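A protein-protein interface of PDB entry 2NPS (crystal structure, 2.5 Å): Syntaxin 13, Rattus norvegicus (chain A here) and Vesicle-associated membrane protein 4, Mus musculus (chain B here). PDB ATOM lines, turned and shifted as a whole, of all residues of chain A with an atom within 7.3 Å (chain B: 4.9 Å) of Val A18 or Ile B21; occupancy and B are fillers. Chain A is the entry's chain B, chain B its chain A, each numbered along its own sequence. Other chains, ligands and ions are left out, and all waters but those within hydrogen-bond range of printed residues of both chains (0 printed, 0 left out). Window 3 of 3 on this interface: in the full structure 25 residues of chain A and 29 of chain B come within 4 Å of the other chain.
The side-chain carboxylate of Asp A14 lies close to the side-chain carboxylate of Asp B18 (3.3 Å).
The backbone carbonyl oxygen (O) of Ile B21 sits at hydrogen-bond distance from the side-chain amide nitrogen (NE2) of Gln B25 (3.0 Å).
Ile B21 touches Val A18.
CB of Met B24 touches CG2 of Ile A21, at 3.5 Å.
Phe A22 touches Val B20.
Phe A22 touches Met B24.
Of chain B, only Ile B21 (3.8 Å) comes within 4 Å of Val A18.
Ile B21 touches one residue of chain A.
Printed residues of chain B within 4 Å of Ile A21: Met B24.
Of the printed residues of chain A, Val B20 touches Phe A22 (3.9 Å).
Of the printed residues of chain A, Asp B18 touches Asp A14.
Printed residues of chain A within 4 Å of Met B24: Ile A21 and Phe A22.
Asp A17 touches none of the printed residues of chain B.
Leu A16 touches none of the printed residues of chain B.
The nearest printed residue of chain B that does not touch Phe A22 is Ile B21 (6.6 Å).
Of the 14 printed residues of chain A, 4 touch a printed residue of chain B.
Printed residues of chain A that touch a printed residue of chain B: Asp A14, Val A18, Ile A21 and Phe A22.
Among the printed residues, no Asp or Glu carboxylate lies within 4 Å of a Lys or Arg side-chain nitrogen of the other chain.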
ATOM      1  N   LEU A  11     -25.399  -8.917 -23.861  1.00  0.00           N
ATOM      2  CA  LEU A  11     -25.027  -8.753 -25.257  1.00  0.00           C
ATOM      3  C   LEU A  11     -25.437  -7.394 -25.810  1.00  0.00           C
ATOM      4  O   LEU A  11     -24.592  -6.650 -26.313  1.00  0.00           O
ATOM      5  CB  LEU A  11     -25.670  -9.843 -26.104  1.00  0.00           C
ATOM      6  CG  LEU A  11     -25.434  -9.692 -27.599  1.00  0.00           C
ATOM      7  CD1 LEU A  11     -23.934  -9.670 -27.871  1.00  0.00           C
ATOM      8  CD2 LEU A  11     -26.106 -10.829 -28.351  1.00  0.00           C
ATOM      9  N   GLU A  12     -26.727  -7.078 -25.724  1.00  0.00           N
ATOM     10  CA  GLU A  12     -27.234  -5.811 -26.235  1.00  0.00           C
ATOM     11  C   GLU A  12     -26.628  -4.629 -25.489  1.00  0.00           C
ATOM     12  O   GLU A  12     -26.286  -3.608 -26.092  1.00  0.00           O
ATOM     13  CB  GLU A  12     -28.754  -5.746 -26.129  1.00  0.00           C
ATOM     14  CG  GLU A  12     -29.323  -4.547 -26.861  1.00  0.00           C
ATOM     15  CD  GLU A  12     -30.670  -4.106 -26.332  1.00  0.00           C
ATOM     16  OE1 GLU A  12     -30.961  -4.367 -25.142  1.00  0.00           O
ATOM     17  OE2 GLU A  12     -31.427  -3.473 -27.102  1.00  0.00           O
ATOM     18  N   ALA A  13     -26.498  -4.773 -24.175  1.00  0.00           N
ATOM     19  CA  ALA A  13     -25.899  -3.731 -23.362  1.00  0.00           C
ATOM     20  C   ALA A  13     -24.493  -3.510 -23.896  1.00  0.00           C
ATOM     21  O   ALA A  13     -24.074  -2.385 -24.137  1.00  0.00           O
ATOM     22  CB  ALA A  13     -25.842  -4.163 -21.900  1.00  0.00           C
ATOM     23  N   ASP A  14     -23.768  -4.602 -24.090  1.00  0.00           N
ATOM     24  CA  ASP A  14     -22.416  -4.505 -24.598  1.00  0.00           C
ATOM     25  C   ASP A  14     -22.372  -3.967 -26.024  1.00  0.00           C
ATOM     26  O   ASP A  14     -21.411  -3.307 -26.414  1.00  0.00           O
ATOM     27  CB  ASP A  14     -21.720  -5.854 -24.479  1.00  0.00           C
ATOM     28  CG  ASP A  14     -21.248  -6.128 -23.051  1.00  0.00           C
ATOM     29  OD1 ASP A  14     -20.694  -7.220 -22.777  1.00  0.00           O
ATOM     30  OD2 ASP A  14     -21.429  -5.233 -22.188  1.00  0.00           O
ATOM     31  N   ILE A  15     -23.421  -4.214 -26.800  1.00  0.00           N
ATOM     32  CA  ILE A  15     -23.453  -3.681 -28.152  1.00  0.00           C
ATOM     33  C   ILE A  15     -23.628  -2.173 -28.057  1.00  0.00           C
ATOM     34  O   ILE A  15     -23.144  -1.434 -28.910  1.00  0.00           O
ATOM     35  CB  ILE A  15     -24.599  -4.275 -29.001  1.00  0.00           C
ATOM     36  CG1 ILE A  15     -24.253  -5.719 -29.403  1.00  0.00           C
ATOM     37  CG2 ILE A  15     -24.819  -3.415 -30.244  1.00  0.00           C
ATOM     38  CD1 ILE A  15     -25.314  -6.397 -30.267  1.00  0.00           C
ATOM     39  N   LEU A  16     -24.313  -1.710 -27.017  1.00  0.00           N
ATOM     40  CA  LEU A  16     -24.500  -0.272 -26.844  1.00  0.00           C
ATOM     41  C   LEU A  16     -23.172   0.372 -26.494  1.00  0.00           C
ATOM     42  O   LEU A  16     -22.929   1.531 -26.806  1.00  0.00           O
ATOM     43  CB  LEU A  16     -25.504   0.027 -25.732  1.00  0.00           C
ATOM     44  CG  LEU A  16     -26.916   0.307 -26.218  1.00  0.00           C
ATOM     45  CD1 LEU A  16     -27.786   0.729 -25.042  1.00  0.00           C
ATOM     46  CD2 LEU A  16     -26.881   1.410 -27.260  1.00  0.00           C
ATOM     47  N   ASP A  17     -22.325  -0.396 -25.822  1.00  0.00           N
ATOM     48  CA  ASP A  17     -21.012   0.073 -25.422  1.00  0.00           C
ATOM     49  C   ASP A  17     -20.190   0.376 -26.651  1.00  0.00           C
ATOM     50  O   ASP A  17     -19.610   1.451 -26.754  1.00  0.00           O
ATOM     51  CB  ASP A  17     -20.299  -0.986 -24.585  1.00  0.00           C
ATOM     52  CG  ASP A  17     -20.590  -0.847 -23.099  1.00  0.00           C
ATOM     53  OD1 ASP A  17     -21.568  -0.149 -22.741  1.00  0.00           O
ATOM     54  OD2 ASP A  17     -19.846  -1.444 -22.283  1.00  0.00           O
ATOM     55  N   VAL A  18     -20.139  -0.570 -27.585  1.00  0.00           N
ATOM     56  CA  VAL A  18     -19.365  -0.360 -28.792  1.00  0.00           C
ATOM     57  C   VAL A  18     -19.894   0.893 -29.474  1.00  0.00           C
ATOM     58  O   VAL A  18     -19.125   1.787 -29.822  1.00  0.00           O
ATOM     59  CB  VAL A  18     -19.437  -1.576 -29.759  1.00  0.00           C
ATOM     60  CG1 VAL A  18     -19.242  -2.854 -28.987  1.00  0.00           C
ATOM     61  CG2 VAL A  18     -20.752  -1.610 -30.501  1.00  0.00           C
ATOM     62  N   ASN A  19     -21.211   0.983 -29.627  1.00  0.00           N
ATOM     63  CA  ASN A  19     -21.793   2.143 -30.278  1.00  0.00           C
ATOM     64  C   ASN A  19     -21.325   3.413 -29.601  1.00  0.00           C
ATOM     65  O   ASN A  19     -21.072   4.421 -30.259  1.00  0.00           O
ATOM     66  CB  ASN A  19     -23.318   2.076 -30.257  1.00  0.00           C
ATOM     67  CG  ASN A  19     -23.954   3.236 -31.005  1.00  0.00           C
ATOM     68  OD1 ASN A  19     -24.178   4.307 -30.444  1.00  0.00           O
ATOM     69  ND2 ASN A  19     -24.229   3.031 -32.286  1.00  0.00           N
ATOM     70  N   GLN A  20     -21.200   3.359 -28.283  1.00  0.00           N
ATOM     71  CA  GLN A  20     -20.752   4.517 -27.551  1.00  0.00           C
ATOM     72  C   GLN A  20     -19.276   4.773 -27.839  1.00  0.00           C
ATOM     73  O   GLN A  20     -18.895   5.881 -28.207  1.00  0.00           O
ATOM     74  CB  GLN A  20     -20.994   4.318 -26.051  1.00  0.00           C
ATOM     75  CG  GLN A  20     -20.685   5.546 -25.195  1.00  0.00           C
ATOM     76  CD  GLN A  20     -21.146   6.845 -25.848  1.00  0.00           C
ATOM     77  OE1 GLN A  20     -22.283   6.952 -26.307  1.00  0.00           O
ATOM     78  NE2 GLN A  20     -20.262   7.839 -25.888  1.00  0.00           N
ATOM     79  N   ILE A  21     -18.448   3.741 -27.699  1.00  0.00           N
ATOM     80  CA  ILE A  21     -17.025   3.895 -27.939  1.00  0.00           C
ATOM     81  C   ILE A  21     -16.768   4.381 -29.362  1.00  0.00           C
ATOM     82  O   ILE A  21     -15.861   5.169 -29.596  1.00  0.00           O
ATOM     83  CB  ILE A  21     -16.259   2.572 -27.700  1.00  0.00           C
ATOM     84  CG1 ILE A  21     -16.645   1.973 -26.348  1.00  0.00           C
ATOM     85  CG2 ILE A  21     -14.751   2.837 -27.664  1.00  0.00           C
ATOM     86  N   PHE A  22     -17.558   3.911 -30.319  1.00  0.00           N
ATOM     87  CA  PHE A  22     -17.378   4.359 -31.689  1.00  0.00           C
ATOM     88  C   PHE A  22     -17.724   5.836 -31.811  1.00  0.00           C
ATOM     89  O   PHE A  22     -17.038   6.585 -32.501  1.00  0.00           O
ATOM     90  CB  PHE A  22     -18.244   3.564 -32.652  1.00  0.00           C
ATOM     91  CG  PHE A  22     -17.571   2.344 -33.218  1.00  0.00           C
ATOM     92  CD1 PHE A  22     -17.222   1.281 -32.404  1.00  0.00           C
ATOM     93  CD2 PHE A  22     -17.316   2.250 -34.585  1.00  0.00           C
ATOM     94  CE1 PHE A  22     -16.642   0.138 -32.943  1.00  0.00           C
ATOM     95  CE2 PHE A  22     -16.739   1.117 -35.132  1.00  0.00           C
ATOM     96  CZ  PHE A  22     -16.396   0.057 -34.312  1.00  0.00           C
ATOM     97  N   LYS A  23     -18.794   6.269 -31.157  1.00  0.00           N
ATOM     98  CA  LYS A  23     -19.141   7.689 -31.213  1.00  0.00           C
ATOM     99  C   LYS A  23     -17.994   8.443 -30.563  1.00  0.00           C
ATOM    100  O   LYS A  23     -17.472   9.388 -31.142  1.00  0.00           O
ATOM    101  CB  LYS A  23     -20.451   7.976 -30.474  1.00  0.00           C
ATOM    102  CG  LYS A  23     -21.698   7.573 -31.250  1.00  0.00           C
ATOM    103  CD  LYS A  23     -22.972   7.850 -30.460  1.00  0.00           C
ATOM    104  CE  LYS A  23     -24.224   7.357 -31.206  1.00  0.00           C
ATOM    105  NZ  LYS A  23     -24.457   8.107 -32.482  1.00  0.00           N
ATOM    106  N   ASP A  24     -17.583   8.000 -29.377  1.00  0.00           N
ATOM    107  CA  ASP A  24     -16.473   8.631 -28.671  1.00  0.00           C
ATOM    108  C   ASP A  24     -15.243   8.795 -29.558  1.00  0.00           C
ATOM    109  O   ASP A  24     -14.671   9.879 -29.637  1.00  0.00           O
ATOM    110  CB  ASP A  24     -16.098   7.820 -27.432  1.00  0.00           C
ATOM    111  CG  ASP A  24     -17.019   8.095 -26.243  1.00  0.00           C
ATOM    112  OD1 ASP A  24     -17.940   8.948 -26.345  1.00  0.00           O
ATOM    113  OD2 ASP A  24     -16.807   7.446 -25.191  1.00  0.00           O
ATOM    114  N   VAL B  17     -17.939  -9.163 -29.256  1.00  0.00           N
ATOM    115  CA  VAL B  17     -18.204  -7.760 -28.947  1.00  0.00           C
ATOM    116  C   VAL B  17     -17.117  -7.279 -28.027  1.00  0.00           C
ATOM    117  O   VAL B  17     -16.546  -6.219 -28.227  1.00  0.00           O
ATOM    118  CB  VAL B  17     -19.549  -7.590 -28.178  1.00  0.00           C
ATOM    119  N   ASP B  18     -16.861  -8.078 -27.002  1.00  0.00           N
ATOM    120  CA  ASP B  18     -15.853  -7.747 -26.013  1.00  0.00           C
ATOM    121  C   ASP B  18     -14.528  -7.588 -26.717  1.00  0.00           C
ATOM    122  O   ASP B  18     -13.645  -6.887 -26.227  1.00  0.00           O
ATOM    123  CB  ASP B  18     -15.742  -8.845 -24.957  1.00  0.00           C
ATOM    124  CG  ASP B  18     -16.968  -8.925 -24.055  1.00  0.00           C
ATOM    125  OD1 ASP B  18     -17.046  -9.871 -23.241  1.00  0.00           O
ATOM    126  OD2 ASP B  18     -17.856  -8.044 -24.150  1.00  0.00           O
ATOM    127  N   GLU B  19     -14.397  -8.238 -27.870  1.00  0.00           N
ATOM    128  CA  GLU B  19     -13.173  -8.134 -28.651  1.00  0.00           C
ATOM    129  C   GLU B  19     -13.156  -6.751 -29.292  1.00  0.00           C
ATOM    130  O   GLU B  19     -12.184  -6.007 -29.164  1.00  0.00           O
ATOM    131  CB  GLU B  19     -13.125  -9.209 -29.736  1.00  0.00           C
ATOM    132  N   VAL B  20     -14.239  -6.412 -29.985  1.00  0.00           N
ATOM    133  CA  VAL B  20     -14.328  -5.099 -30.614  1.00  0.00           C
ATOM    134  C   VAL B  20     -14.089  -4.025 -29.554  1.00  0.00           C
ATOM    135  O   VAL B  20     -13.408  -3.034 -29.805  1.00  0.00           O
ATOM    136  CB  VAL B  20     -15.705  -4.860 -31.274  1.00  0.00           C
ATOM    137  CG1 VAL B  20     -15.729  -3.499 -31.940  1.00  0.00           C
ATOM    138  CG2 VAL B  20     -15.987  -5.933 -32.301  1.00  0.00           C
ATOM    139  N   ILE B  21     -14.643  -4.238 -28.365  1.00  0.00           N
ATOM    140  CA  ILE B  21     -14.467  -3.294 -27.270  1.00  0.00           C
ATOM    141  C   ILE B  21     -12.988  -3.212 -26.919  1.00  0.00           C
ATOM    142  O   ILE B  21     -12.491  -2.154 -26.547  1.00  0.00           O
ATOM    143  CB  ILE B  21     -15.235  -3.719 -25.998  1.00  0.00           C
ATOM    144  CG1 ILE B  21     -16.745  -3.706 -26.254  1.00  0.00           C
ATOM    145  CG2 ILE B  21     -14.898  -2.771 -24.852  1.00  0.00           C
ATOM    146  N   ASP B  22     -12.290  -4.334 -27.041  1.00  0.00           N
ATOM    147  CA  ASP B  22     -10.868  -4.390 -26.731  1.00  0.00           C
ATOM    148  C   ASP B  22     -10.039  -3.608 -27.739  1.00  0.00           C
ATOM    149  O   ASP B  22      -9.084  -2.932 -27.372  1.00  0.00           O
ATOM    150  CB  ASP B  22     -10.398  -5.836 -26.713  1.00  0.00           C
ATOM    151  CG  ASP B  22      -8.882  -5.953 -26.667  1.00  0.00           C
ATOM    152  OD1 ASP B  22      -8.290  -5.580 -25.619  1.00  0.00           O
ATOM    153  OD2 ASP B  22      -8.285  -6.410 -27.681  1.00  0.00           O
ATOM    154  N   VAL B  23     -10.412  -3.714 -29.008  1.00  0.00           N
ATOM    155  CA  VAL B  23      -9.716  -3.013 -30.080  1.00  0.00           C
ATOM    156  C   VAL B  23      -9.972  -1.507 -29.983  1.00  0.00           C
ATOM    157  O   VAL B  23      -9.056  -0.692 -30.065  1.00  0.00           O
ATOM    158  CB  VAL B  23     -10.207  -3.505 -31.438  1.00  0.00           C
ATOM    159  CG1 VAL B  23      -9.398  -2.869 -32.549  1.00  0.00           C
ATOM    160  CG2 VAL B  23     -10.119  -5.010 -31.502  1.00  0.00           C
ATOM    161  N   MET B  24     -11.238  -1.150 -29.814  1.00  0.00           N
ATOM    162  CA  MET B  24     -11.627   0.249 -29.713  1.00  0.00           C
ATOM    163  C   MET B  24     -10.981   0.925 -28.516  1.00  0.00           C
ATOM    164  O   MET B  24     -10.531   2.068 -28.603  1.00  0.00           O
ATOM    165  CB  MET B  24     -13.148   0.368 -29.617  1.00  0.00           C
ATOM    166  CG  MET B  24     -13.854   0.096 -30.923  1.00  0.00           C
ATOM    167  SD  MET B  24     -13.139   1.104 -32.241  1.00  0.00           S
ATOM    168  CE  MET B  24     -14.060   2.616 -32.082  1.00  0.00           C
ATOM    169  N   GLN B  25     -10.937   0.212 -27.397  1.00  0.00           N
ATOM    170  CA  GLN B  25     -10.336   0.756 -26.196  1.00  0.00           C
ATOM    171  C   GLN B  25      -8.898   1.139 -26.469  1.00  0.00           C
ATOM    172  O   GLN B  25      -8.430   2.177 -26.001  1.00  0.00           O
ATOM    173  CB  GLN B  25     -10.407  -0.254 -25.060  1.00  0.00           C
ATOM    174  CG  GLN B  25     -11.624  -0.058 -24.179  1.00  0.00           C
ATOM    175  CD  GLN B  25     -11.948  -1.273 -23.345  1.00  0.00           C
ATOM    176  OE1 GLN B  25     -12.689  -1.184 -22.361  1.00  0.00           O
ATOM    177  NE2 GLN B  25     -11.415  -2.424 -23.743  1.00  0.00           N
